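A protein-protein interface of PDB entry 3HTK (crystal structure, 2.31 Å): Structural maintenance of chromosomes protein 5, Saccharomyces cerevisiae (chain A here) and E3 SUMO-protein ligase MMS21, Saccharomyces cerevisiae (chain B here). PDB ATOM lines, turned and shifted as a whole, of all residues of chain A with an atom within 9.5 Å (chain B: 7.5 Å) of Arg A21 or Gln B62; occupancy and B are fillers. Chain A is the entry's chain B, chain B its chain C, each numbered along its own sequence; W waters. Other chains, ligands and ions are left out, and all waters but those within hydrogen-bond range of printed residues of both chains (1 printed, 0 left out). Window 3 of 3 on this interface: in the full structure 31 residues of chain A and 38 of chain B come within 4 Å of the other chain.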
ATOM      1  N   ASP A  11     -24.426  24.737  14.478  1.00  0.00           N
ATOM      2  CA  ASP A  11     -23.970  23.661  15.351  1.00  0.00           C
ATOM      3  C   ASP A  11     -25.184  23.014  16.007  1.00  0.00           C
ATOM      4  O   ASP A  11     -25.272  21.786  16.113  1.00  0.00           O
ATOM      5  CB  ASP A  11     -23.040  24.197  16.439  1.00  0.00           C
ATOM      6  CG  ASP A  11     -22.912  23.238  17.615  1.00  0.00           C
ATOM      7  OD1 ASP A  11     -22.442  22.092  17.408  1.00  0.00           O
ATOM      8  OD2 ASP A  11     -23.293  23.629  18.744  1.00  0.00           O
ATOM      9  N   ILE A  13     -28.032  22.791  14.830  1.00  0.00           N
ATOM     10  CA  ILE A  13     -28.632  21.966  13.786  1.00  0.00           C
ATOM     11  C   ILE A  13     -27.940  20.609  13.808  1.00  0.00           C
ATOM     12  O   ILE A  13     -28.581  19.578  13.645  1.00  0.00           O
ATOM     13  CB  ILE A  13     -28.416  22.549  12.354  1.00  0.00           C
ATOM     14  CG1 ILE A  13     -28.972  23.977  12.239  1.00  0.00           C
ATOM     15  CG2 ILE A  13     -29.070  21.626  11.323  1.00  0.00           C
ATOM     16  CD1 ILE A  13     -30.446  24.068  11.949  1.00  0.00           C
ATOM     17  N   GLN A  14     -26.623  20.620  13.998  1.00  0.00           N
ATOM     18  CA  GLN A  14     -25.848  19.383  14.012  1.00  0.00           C
ATOM     19  C   GLN A  14     -26.146  18.531  15.243  1.00  0.00           C
ATOM     20  O   GLN A  14     -26.189  17.305  15.150  1.00  0.00           O
ATOM     21  CB  GLN A  14     -24.341  19.676  13.929  1.00  0.00           C
ATOM     22  CG  GLN A  14     -23.910  20.526  12.724  1.00  0.00           C
ATOM     23  CD  GLN A  14     -24.519  20.070  11.406  1.00  0.00           C
ATOM     24  OE1 GLN A  14     -24.471  18.886  11.055  1.00  0.00           O
ATOM     25  NE2 GLN A  14     -25.089  21.018  10.660  1.00  0.00           N
ATOM     26  N   GLN A  15     -26.349  19.173  16.391  1.00  0.00           N
ATOM     27  CA  GLN A  15     -26.670  18.424  17.604  1.00  0.00           C
ATOM     28  C   GLN A  15     -28.045  17.783  17.460  1.00  0.00           C
ATOM     29  O   GLN A  15     -28.282  16.688  17.963  1.00  0.00           O
ATOM     30  CB  GLN A  15     -26.667  19.332  18.835  1.00  0.00           C
ATOM     31  CG  GLN A  15     -25.308  19.840  19.196  1.00  0.00           C
ATOM     32  CD  GLN A  15     -24.261  18.753  19.114  1.00  0.00           C
ATOM     33  OE1 GLN A  15     -24.378  17.709  19.763  1.00  0.00           O
ATOM     34  NE2 GLN A  15     -23.227  18.990  18.310  1.00  0.00           N
ATOM     35  N   LEU A  16     -28.950  18.477  16.771  1.00  0.00           N
ATOM     36  CA  LEU A  16     -30.298  17.960  16.556  1.00  0.00           C
ATOM     37  C   LEU A  16     -30.303  16.824  15.549  1.00  0.00           C
ATOM     38  O   LEU A  16     -31.104  15.897  15.656  1.00  0.00           O
ATOM     39  CB  LEU A  16     -31.227  19.063  16.063  1.00  0.00           C
ATOM     40  CG  LEU A  16     -31.526  20.139  17.094  1.00  0.00           C
ATOM     41  CD1 LEU A  16     -32.563  21.117  16.537  1.00  0.00           C
ATOM     42  CD2 LEU A  16     -32.029  19.470  18.360  1.00  0.00           C
ATOM     43  N   LEU A  17     -29.420  16.914  14.559  1.00  0.00           N
ATOM     44  CA  LEU A  17     -29.332  15.881  13.543  1.00  0.00           C
ATOM     45  C   LEU A  17     -28.804  14.618  14.206  1.00  0.00           C
ATOM     46  O   LEU A  17     -29.167  13.514  13.817  1.00  0.00           O
ATOM     47  CB  LEU A  17     -28.405  16.318  12.398  1.00  0.00           C
ATOM     48  CG  LEU A  17     -28.956  17.407  11.463  1.00  0.00           C
ATOM     49  CD1 LEU A  17     -27.943  17.737  10.361  1.00  0.00           C
ATOM     50  CD2 LEU A  17     -30.253  16.922  10.852  1.00  0.00           C
ATOM     51  N   LEU A  18     -27.944  14.786  15.209  1.00  0.00           N
ATOM     52  CA  LEU A  18     -27.408  13.639  15.928  1.00  0.00           C
ATOM     53  C   LEU A  18     -28.547  13.017  16.729  1.00  0.00           C
ATOM     54  O   LEU A  18     -28.806  11.819  16.601  1.00  0.00           O
ATOM     55  CB  LEU A  18     -26.286  14.051  16.880  1.00  0.00           C
ATOM     56  CG  LEU A  18     -25.552  12.853  17.507  1.00  0.00           C
ATOM     57  CD1 LEU A  18     -24.956  11.998  16.401  1.00  0.00           C
ATOM     58  CD2 LEU A  18     -24.450  13.331  18.450  1.00  0.00           C
ATOM     59  N   LYS A  19     -29.230  13.833  17.540  1.00  0.00           N
ATOM     60  CA  LYS A  19     -30.351  13.347  18.350  1.00  0.00           C
ATOM     61  C   LYS A  19     -31.337  12.532  17.521  1.00  0.00           C
ATOM     62  O   LYS A  19     -31.902  11.558  17.999  1.00  0.00           O
ATOM     63  CB  LYS A  19     -31.096  14.502  19.026  1.00  0.00           C
ATOM     64  CG  LYS A  19     -30.456  14.960  20.329  1.00  0.00           C
ATOM     65  CD  LYS A  19     -31.393  15.864  21.129  1.00  0.00           C
ATOM     66  CE  LYS A  19     -30.801  16.207  22.498  1.00  0.00           C
ATOM     67  NZ  LYS A  19     -31.707  17.071  23.320  1.00  0.00           N
ATOM     68  N   GLN A  20     -31.550  12.935  16.278  1.00  0.00           N
ATOM     69  CA  GLN A  20     -32.449  12.195  15.417  1.00  0.00           C
ATOM     70  C   GLN A  20     -31.918  10.786  15.219  1.00  0.00           C
ATOM     71  O   GLN A  20     -32.663   9.814  15.294  1.00  0.00           O
ATOM     72  CB  GLN A  20     -32.571  12.861  14.054  1.00  0.00           C
ATOM     73  CG  GLN A  20     -33.412  14.101  14.039  1.00  0.00           C
ATOM     74  CD  GLN A  20     -33.561  14.642  12.639  1.00  0.00           C
ATOM     75  OE1 GLN A  20     -33.882  13.900  11.708  1.00  0.00           O
ATOM     76  NE2 GLN A  20     -33.329  15.942  12.478  1.00  0.00           N
ATOM     77  N   ARG A  21     -30.624  10.674  14.964  1.00  0.00           N
ATOM     78  CA  ARG A  21     -30.046   9.364  14.736  1.00  0.00           C
ATOM     79  C   ARG A  21     -30.176   8.479  15.973  1.00  0.00           C
ATOM     80  O   ARG A  21     -30.412   7.277  15.851  1.00  0.00           O
ATOM     81  CB  ARG A  21     -28.586   9.501  14.267  1.00  0.00           C
ATOM     82  CG  ARG A  21     -28.477  10.147  12.884  1.00  0.00           C
ATOM     83  CD  ARG A  21     -27.061  10.071  12.297  1.00  0.00           C
ATOM     84  NE  ARG A  21     -26.081  10.889  13.015  1.00  0.00           N
ATOM     85  CZ  ARG A  21     -25.949  12.211  12.887  1.00  0.00           C
ATOM     86  NH1 ARG A  21     -26.733  12.895  12.060  1.00  0.00           N
ATOM     87  NH2 ARG A  21     -25.028  12.856  13.594  1.00  0.00           N
ATOM     88  N   HIS A  22     -30.057   9.076  17.160  1.00  0.00           N
ATOM     89  CA  HIS A  22     -30.196   8.319  18.406  1.00  0.00           C
ATOM     90  C   HIS A  22     -31.640   7.817  18.583  1.00  0.00           C
ATOM     91  O   HIS A  22     -31.863   6.632  18.822  1.00  0.00           O
ATOM     92  CB  HIS A  22     -29.805   9.189  19.603  1.00  0.00           C
ATOM     93  CG  HIS A  22     -28.327   9.334  19.795  1.00  0.00           C
ATOM     94  ND1 HIS A  22     -27.406   8.896  18.866  1.00  0.00           N
ATOM     95  CD2 HIS A  22     -27.610   9.893  20.800  1.00  0.00           C
ATOM     96  CE1 HIS A  22     -26.187   9.180  19.290  1.00  0.00           C
ATOM     97  NE2 HIS A  22     -26.284   9.787  20.460  1.00  0.00           N
ATOM     98  N   LEU A  23     -32.608   8.725  18.468  1.00  0.00           N
ATOM     99  CA  LEU A  23     -34.031   8.385  18.592  1.00  0.00           C
ATOM    100  C   LEU A  23     -34.471   7.355  17.552  1.00  0.00           C
ATOM    101  O   LEU A  23     -35.406   6.580  17.774  1.00  0.00           O
ATOM    102  CB  LEU A  23     -34.893   9.639  18.428  1.00  0.00           C
ATOM    103  CG  LEU A  23     -34.992  10.561  19.635  1.00  0.00           C
ATOM    104  CD1 LEU A  23     -35.680  11.869  19.242  1.00  0.00           C
ATOM    105  CD2 LEU A  23     -35.774   9.859  20.736  1.00  0.00           C
ATOM    106  N   LEU A  24     -33.803   7.365  16.404  1.00  0.00           N
ATOM    107  CA  LEU A  24     -34.132   6.432  15.334  1.00  0.00           C
ATOM    108  C   LEU A  24     -33.717   5.035  15.824  1.00  0.00           C
ATOM    109  O   LEU A  24     -34.383   4.028  15.544  1.00  0.00           O
ATOM    110  CB  LEU A  24     -33.379   6.850  14.068  1.00  0.00           C
ATOM    111  CG  LEU A  24     -34.029   6.850  12.681  1.00  0.00           C
ATOM    112  CD1 LEU A  24     -35.533   7.317  12.659  1.00  0.00           C
ATOM    113  CD2 LEU A  24     -33.150   7.766  11.837  1.00  0.00           C
ATOM    114  N   SER A  25     -32.619   4.994  16.571  1.00  0.00           N
ATOM    115  CA  SER A  25     -32.129   3.751  17.146  1.00  0.00           C
ATOM    116  C   SER A  25     -33.136   3.252  18.194  1.00  0.00           C
ATOM    117  O   SER A  25     -33.456   2.066  18.236  1.00  0.00           O
ATOM    118  CB  SER A  25     -30.772   3.982  17.800  1.00  0.00           C
ATOM    119  OG  SER A  25     -30.223   2.764  18.257  1.00  0.00           O
ATOM    120  N   LYS A  26     -33.634   4.162  19.031  1.00  0.00           N
ATOM    121  CA  LYS A  26     -34.627   3.818  20.057  1.00  0.00           C
ATOM    122  C   LYS A  26     -35.895   3.276  19.388  1.00  0.00           C
ATOM    123  O   LYS A  26     -36.471   2.277  19.816  1.00  0.00           O
ATOM    124  CB  LYS A  26     -34.988   5.051  20.884  1.00  0.00           C
ATOM    125  CG  LYS A  26     -33.897   5.528  21.815  1.00  0.00           C
ATOM    126  CD  LYS A  26     -33.656   4.526  22.934  1.00  0.00           C
ATOM    127  CE  LYS A  26     -32.661   5.071  23.964  1.00  0.00           C
ATOM    128  NZ  LYS A  26     -32.454   4.112  25.097  1.00  0.00           N
ATOM    129  N   MET A  27     -36.319   3.956  18.332  1.00  0.00           N
ATOM    130  CA  MET A  27     -37.493   3.572  17.568  1.00  0.00           C
ATOM    131  C   MET A  27     -37.425   2.103  17.119  1.00  0.00           C
ATOM    132  O   MET A  27     -38.397   1.362  17.244  1.00  0.00           O
ATOM    133  CB  MET A  27     -37.618   4.498  16.354  1.00  0.00           C
ATOM    134  CG  MET A  27     -38.729   4.148  15.412  1.00  0.00           C
ATOM    135  SD  MET A  27     -38.709   5.224  13.974  1.00  0.00           S
ATOM    136  CE  MET A  27     -37.624   4.297  12.906  1.00  0.00           C
ATOM    137  N   ALA A  28     -36.280   1.694  16.581  1.00  0.00           N
ATOM    138  CA  ALA A  28     -36.087   0.314  16.129  1.00  0.00           C
ATOM    139  C   ALA A  28     -36.137  -0.657  17.313  1.00  0.00           C
ATOM    140  O   ALA A  28     -36.678  -1.759  17.207  1.00  0.00           O
ATOM    141  CB  ALA A  28     -34.750   0.183  15.412  1.00  0.00           C
ATOM    142  N   SER A  29     -35.555  -0.237  18.433  1.00  0.00           N
ATOM    143  CA  SER A  29     -35.532  -1.042  19.647  1.00  0.00           C
ATOM    144  C   SER A  29     -36.973  -1.203  20.123  1.00  0.00           C
ATOM    145  O   SER A  29     -37.394  -2.287  20.540  1.00  0.00           O
ATOM    146  CB  SER A  29     -34.719  -0.325  20.721  1.00  0.00           C
ATOM    147  OG  SER A  29     -34.855  -0.949  21.986  1.00  0.00           O
ATOM    148  N   THR B  44     -35.186  11.565   7.774  1.00  0.00           N
ATOM    149  CA  THR B  44     -33.938  11.803   8.489  1.00  0.00           C
ATOM    150  C   THR B  44     -32.773  11.982   7.522  1.00  0.00           C
ATOM    151  O   THR B  44     -31.862  12.768   7.790  1.00  0.00           O
ATOM    152  CB  THR B  44     -33.626  10.661   9.477  1.00  0.00           C
ATOM    153  OG1 THR B  44     -34.581  10.688  10.544  1.00  0.00           O
ATOM    154  CG2 THR B  44     -32.224  10.807  10.057  1.00  0.00           C
ATOM    155  N   LEU B  48     -30.664  15.357   6.928  1.00  0.00           N
ATOM    156  CA  LEU B  48     -29.244  15.079   7.070  1.00  0.00           C
ATOM    157  C   LEU B  48     -28.538  15.704   5.869  1.00  0.00           C
ATOM    158  O   LEU B  48     -27.636  16.515   6.022  1.00  0.00           O
ATOM    159  CB  LEU B  48     -29.011  13.566   7.104  1.00  0.00           C
ATOM    160  CG  LEU B  48     -27.657  13.018   7.566  1.00  0.00           C
ATOM    161  CD1 LEU B  48     -26.594  13.283   6.515  1.00  0.00           C
ATOM    162  CD2 LEU B  48     -27.276  13.637   8.901  1.00  0.00           C
ATOM    163  N   THR B  52     -26.523  19.133   6.845  1.00  0.00           N
ATOM    164  CA  THR B  52     -25.221  18.761   7.379  1.00  0.00           C
ATOM    165  C   THR B  52     -24.207  19.865   7.100  1.00  0.00           C
ATOM    166  O   THR B  52     -24.142  20.399   5.994  1.00  0.00           O
ATOM    167  CB  THR B  52     -24.704  17.447   6.781  1.00  0.00           C
ATOM    168  OG1 THR B  52     -25.585  16.384   7.149  1.00  0.00           O
ATOM    169  CG2 THR B  52     -23.316  17.126   7.325  1.00  0.00           C
ATOM    170  N   SER B  53     -23.434  20.204   8.128  1.00  0.00           N
ATOM    171  CA  SER B  53     -22.404  21.233   8.054  1.00  0.00           C
ATOM    172  C   SER B  53     -21.372  20.872   6.980  1.00  0.00           C
ATOM    173  O   SER B  53     -21.064  19.697   6.777  1.00  0.00           O
ATOM    174  CB  SER B  53     -21.722  21.361   9.424  1.00  0.00           C
ATOM    175  OG  SER B  53     -20.790  22.427   9.463  1.00  0.00           O
ATOM    176  N   ILE B  57     -15.498  15.353   5.274  1.00  0.00           N
ATOM    177  CA  ILE B  57     -15.574  14.332   6.311  1.00  0.00           C
ATOM    178  C   ILE B  57     -16.322  13.098   5.816  1.00  0.00           C
ATOM    179  O   ILE B  57     -16.664  12.212   6.598  1.00  0.00           O
ATOM    180  CB  ILE B  57     -16.266  14.865   7.579  1.00  0.00           C
ATOM    181  CG1 ILE B  57     -16.301  13.784   8.661  1.00  0.00           C
ATOM    182  CG2 ILE B  57     -17.672  15.347   7.256  1.00  0.00           C
ATOM    183  CD1 ILE B  57     -14.961  13.533   9.317  1.00  0.00           C
ATOM    184  N   GLY B  58     -16.571  13.048   4.511  1.00  0.00           N
ATOM    185  CA  GLY B  58     -17.924  12.946   3.997  1.00  0.00           C
ATOM    186  C   GLY B  58     -18.958  12.846   5.101  1.00  0.00           C
ATOM    187  O   GLY B  58     -18.886  13.561   6.100  1.00  0.00           O
ATOM    188  N   ILE B  59     -19.925  11.952   4.920  1.00  0.00           N
ATOM    189  CA  ILE B  59     -20.912  11.671   5.955  1.00  0.00           C
ATOM    190  C   ILE B  59     -20.965  10.181   6.277  1.00  0.00           C
ATOM    191  O   ILE B  59     -22.013   9.654   6.649  1.00  0.00           O
ATOM    192  CB  ILE B  59     -22.317  12.146   5.540  1.00  0.00           C
ATOM    193  CG1 ILE B  59     -22.524  11.950   4.036  1.00  0.00           C
ATOM    194  CG2 ILE B  59     -22.521  13.603   5.924  1.00  0.00           C
ATOM    195  CD1 ILE B  59     -23.957  12.130   3.587  1.00  0.00           C
ATOM    196  N   GLU B  60     -19.828   9.509   6.131  1.00  0.00           N
ATOM    197  CA  GLU B  60     -19.796   8.051   6.116  1.00  0.00           C
ATOM    198  C   GLU B  60     -20.292   7.476   7.439  1.00  0.00           C
ATOM    199  O   GLU B  60     -20.891   6.400   7.473  1.00  0.00           O
ATOM    200  CB  GLU B  60     -18.380   7.549   5.822  1.00  0.00           C
ATOM    201  CG  GLU B  60     -17.761   8.140   4.567  1.00  0.00           C
ATOM    202  CD  GLU B  60     -16.271   7.876   4.472  1.00  0.00           C
ATOM    203  OE1 GLU B  60     -15.500   8.544   5.193  1.00  0.00           O
ATOM    204  OE2 GLU B  60     -15.871   7.000   3.678  1.00  0.00           O
ATOM    205  N   GLU B  61     -20.039   8.198   8.525  1.00  0.00           N
ATOM    206  CA  GLU B  61     -20.496   7.783   9.844  1.00  0.00           C
ATOM    207  C   GLU B  61     -22.025   7.797   9.913  1.00  0.00           C
ATOM    208  O   GLU B  61     -22.663   6.753  10.076  1.00  0.00           O
ATOM    209  CB  GLU B  61     -19.903   8.741  10.874  1.00  0.00           C
ATOM    210  CG  GLU B  61     -20.015   8.306  12.306  1.00  0.00           C
ATOM    211  CD  GLU B  61     -18.832   8.792  13.113  1.00  0.00           C
ATOM    212  OE1 GLU B  61     -18.602  10.022  13.150  1.00  0.00           O
ATOM    213  OE2 GLU B  61     -18.127   7.941  13.700  1.00  0.00           O
ATOM    214  N   GLN B  62     -22.594   8.994   9.792  1.00  0.00           N
ATOM    215  CA  GLN B  62     -24.037   9.204   9.805  1.00  0.00           C
ATOM    216  C   GLN B  62     -24.764   8.149   8.982  1.00  0.00           C
ATOM    217  O   GLN B  62     -25.735   7.563   9.438  1.00  0.00           O
ATOM    218  CB  GLN B  62     -24.387  10.587   9.236  1.00  0.00           C
ATOM    219  CG  GLN B  62     -23.939  11.784  10.061  1.00  0.00           C
ATOM    220  CD  GLN B  62     -22.484  12.214   9.806  1.00  0.00           C
ATOM    221  OE1 GLN B  62     -22.033  13.227  10.351  1.00  0.00           O
ATOM    222  NE2 GLN B  62     -21.757  11.456   8.983  1.00  0.00           N
ATOM    223  N   VAL B  63     -24.294   7.930   7.754  1.00  0.00           N
ATOM    224  CA  VAL B  63     -24.888   6.949   6.854  1.00  0.00           C
ATOM    225  C   VAL B  63     -24.772   5.544   7.416  1.00  0.00           C
ATOM    226  O   VAL B  63     -25.690   4.745   7.284  1.00  0.00           O
ATOM    227  CB  VAL B  63     -24.206   6.967   5.468  1.00  0.00           C
ATOM    228  CG1 VAL B  63     -24.806   5.871   4.562  1.00  0.00           C
ATOM    229  CG2 VAL B  63     -24.364   8.345   4.834  1.00  0.00           C
ATOM    230  N   ALA B  64     -23.639   5.231   8.034  1.00  0.00           N
ATOM    231  CA  ALA B  64     -23.449   3.900   8.610  1.00  0.00           C
ATOM    232  C   ALA B  64     -24.485   3.654   9.713  1.00  0.00           C
ATOM    233  O   ALA B  64     -25.099   2.592   9.763  1.00  0.00           O
ATOM    234  CB  ALA B  64     -22.024   3.755   9.183  1.00  0.00           C
ATOM    235  N   ASP B  65     -24.680   4.642  10.583  1.00  0.00           N
ATOM    236  CA  ASP B  65     -25.634   4.516  11.677  1.00  0.00           C
ATOM    237  C   ASP B  65     -27.058   4.324  11.153  1.00  0.00           C
ATOM    238  O   ASP B  65     -27.745   3.384  11.533  1.00  0.00           O
ATOM    239  CB  ASP B  65     -25.568   5.747  12.583  1.00  0.00           C
ATOM    240  CG  ASP B  65     -26.586   5.692  13.727  1.00  0.00           C
ATOM    241  OD1 ASP B  65     -26.587   6.612  14.572  1.00  0.00           O
ATOM    242  OD2 ASP B  65     -27.387   4.730  13.782  1.00  0.00           O
ATOM    243  N   ILE B  66     -27.487   5.205  10.259  1.00  0.00           N
ATOM    244  CA  ILE B  66     -28.819   5.124   9.689  1.00  0.00           C
ATOM    245  C   ILE B  66     -29.062   3.795   8.987  1.00  0.00           C
ATOM    246  O   ILE B  66     -30.112   3.190   9.152  1.00  0.00           O
ATOM    247  CB  ILE B  66     -29.051   6.283   8.688  1.00  0.00           C
ATOM    248  CG1 ILE B  66     -28.995   7.618   9.429  1.00  0.00           C
ATOM    249  CG2 ILE B  66     -30.384   6.130   7.988  1.00  0.00           C
ATOM    250  CD1 ILE B  66     -29.995   7.745  10.528  1.00  0.00           C
ATOM    251  N   THR B  67     -28.097   3.344   8.198  1.00  0.00           N
ATOM    252  CA  THR B  67     -28.245   2.083   7.476  1.00  0.00           C
ATOM    253  C   THR B  67     -28.308   0.909   8.446  1.00  0.00           C
ATOM    254  O   THR B  67     -28.940  -0.113   8.163  1.00  0.00           O
ATOM    255  CB  THR B  67     -27.074   1.853   6.516  1.00  0.00           C
ATOM    256  OG1 THR B  67     -25.855   1.825   7.265  1.00  0.00           O
ATOM    257  CG2 THR B  67     -26.999   2.973   5.493  1.00  0.00           C
ATOM    258  N   SER B  68     -27.649   1.065   9.588  1.00  0.00           N
ATOM    259  CA  SER B  68     -27.641   0.032  10.614  1.00  0.00           C
ATOM    260  C   SER B  68     -29.048  -0.157  11.190  1.00  0.00           C
ATOM    261  O   SER B  68     -29.493  -1.293  11.366  1.00  0.00           O
ATOM    262  CB  SER B  68     -26.645   0.404  11.723  1.00  0.00           C
ATOM    263  OG  SER B  68     -26.857  -0.342  12.908  1.00  0.00           O
ATOM    264  N   THR B  69     -29.761   0.938  11.472  1.00  0.00           N
ATOM    265  CA  THR B  69     -31.106   0.783  12.014  1.00  0.00           C
ATOM    266  C   THR B  69     -32.073   0.458  10.886  1.00  0.00           C
ATOM    267  O   THR B  69     -33.032  -0.276  11.078  1.00  0.00           O
ATOM    268  CB  THR B  69     -31.622   2.045  12.768  1.00  0.00           C
ATOM    269  OG1 THR B  69     -32.169   2.979  11.836  1.00  0.00           O
ATOM    270  CG2 THR B  69     -30.515   2.692  13.556  1.00  0.00           C
ATOM    271  N   LEU B 147     -28.884   5.343   0.533  1.00  0.00           N
ATOM    272  CA  LEU B 147     -27.928   5.209   1.629  1.00  0.00           C
ATOM    273  C   LEU B 147     -26.590   4.706   1.108  1.00  0.00           C
ATOM    274  O   LEU B 147     -25.536   5.229   1.467  1.00  0.00           O
ATOM    275  CB  LEU B 147     -28.458   4.247   2.688  1.00  0.00           C
ATOM    276  CG  LEU B 147     -29.628   4.735   3.547  1.00  0.00           C
ATOM    277  CD1 LEU B 147     -30.152   3.588   4.401  1.00  0.00           C
ATOM    278  CD2 LEU B 147     -29.168   5.894   4.422  1.00  0.00           C
ATOM    279  N   LEU B 150     -25.251   7.704  -1.235  1.00  0.00           N
ATOM    280  CA  LEU B 150     -25.081   8.952  -0.509  1.00  0.00           C
ATOM    281  C   LEU B 150     -23.677   9.365  -0.084  1.00  0.00           C
ATOM    282  O   LEU B 150     -23.225  10.470  -0.397  1.00  0.00           O
ATOM    283  CB  LEU B 150     -26.001   8.975   0.712  1.00  0.00           C
ATOM    284  CG  LEU B 150     -26.035  10.284   1.505  1.00  0.00           C
ATOM    285  CD1 LEU B 150     -26.209  11.467   0.569  1.00  0.00           C
ATOM    286  CD2 LEU B 150     -27.177  10.238   2.511  1.00  0.00           C
HETATM  287  O   HOH W   1     -24.055   8.959  14.168  1.00  0.00           O
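Hydrophobic or aromatic side chains of chain A within 4 Å of the printed part of chain B: Leu A24.
Of the 19 printed residues of chain B, 7 touch a printed residue of chain A.
Printed residues of chain B that touch a printed residue of chain A: Thr B44, Leu B48, Thr B52, Ser B53, Gln B62, Asp B65 and Ile B66.
Hydrophobic or aromatic side chains of chain B within 4 Å of the printed part of chain A: Leu B48 and Ile B66.
Among the printed residues, no Asp or Glu carboxylate lies within 4 Å of a Lys or Arg side-chain nitrogen of the other chain.
O of Ile B66 is in hydrogen-bond range of OG1 of Thr B69, 3.4 Å away.
NE2 of Gln B62 is in hydrogen-bond range of O of Ile B59.
The backbone carbonyl oxygen (O) of Leu A17 is in hydrogen-bond range of the guanidinium group (NH1) of Arg A21, 3.1 Å away.
The side-chain amide oxygen (OE1) of Gln A20 sits at hydrogen-bond distance from the side-chain hydroxyl (OG1) of Thr B44.
N of Ser B53 lies close to NE2 of Gln A14, at 3.1 Å.
Water W1 bridges NE of Arg A21 (3.0 Å) and OD1 of Asp B65 (3.5 Å).
Among the printed residues, merely in contact across the chains: Gln A14 with Thr B52, Arg A21 with Leu B48, Arg A21 with Gln B62, Arg A21 with Asp B65, Arg A21 with Ile B66, Leu A24 with Thr B44 and Leu A24 with Ile B66.
Printed residues of chain B within 4 Å of Gln A14: Thr B52 and Ser B53.
Of chain B, only Leu B48, Gln B62, Asp B65 and Ile B66 come within 4 Å of Arg A21.
Printed residues of chain A within 4 Å of Thr B44: Gln A20 and Leu A24.
Printed residues of chain A within 4 Å of Leu B48: Arg A21.
Gln B62 touches just one residue of chain A: Arg A21 (3.5 Å).
No residue of chain A comes within 4 Å of Val B63.
No residue of chain A comes within 4 Å of Ala B64.
Asp B65 touches just one residue of chain A: Arg A21 (3.5 Å).
The nearest printed residue of chain B that does not touch Gln A20 is Ile B66 (5.8 Å).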
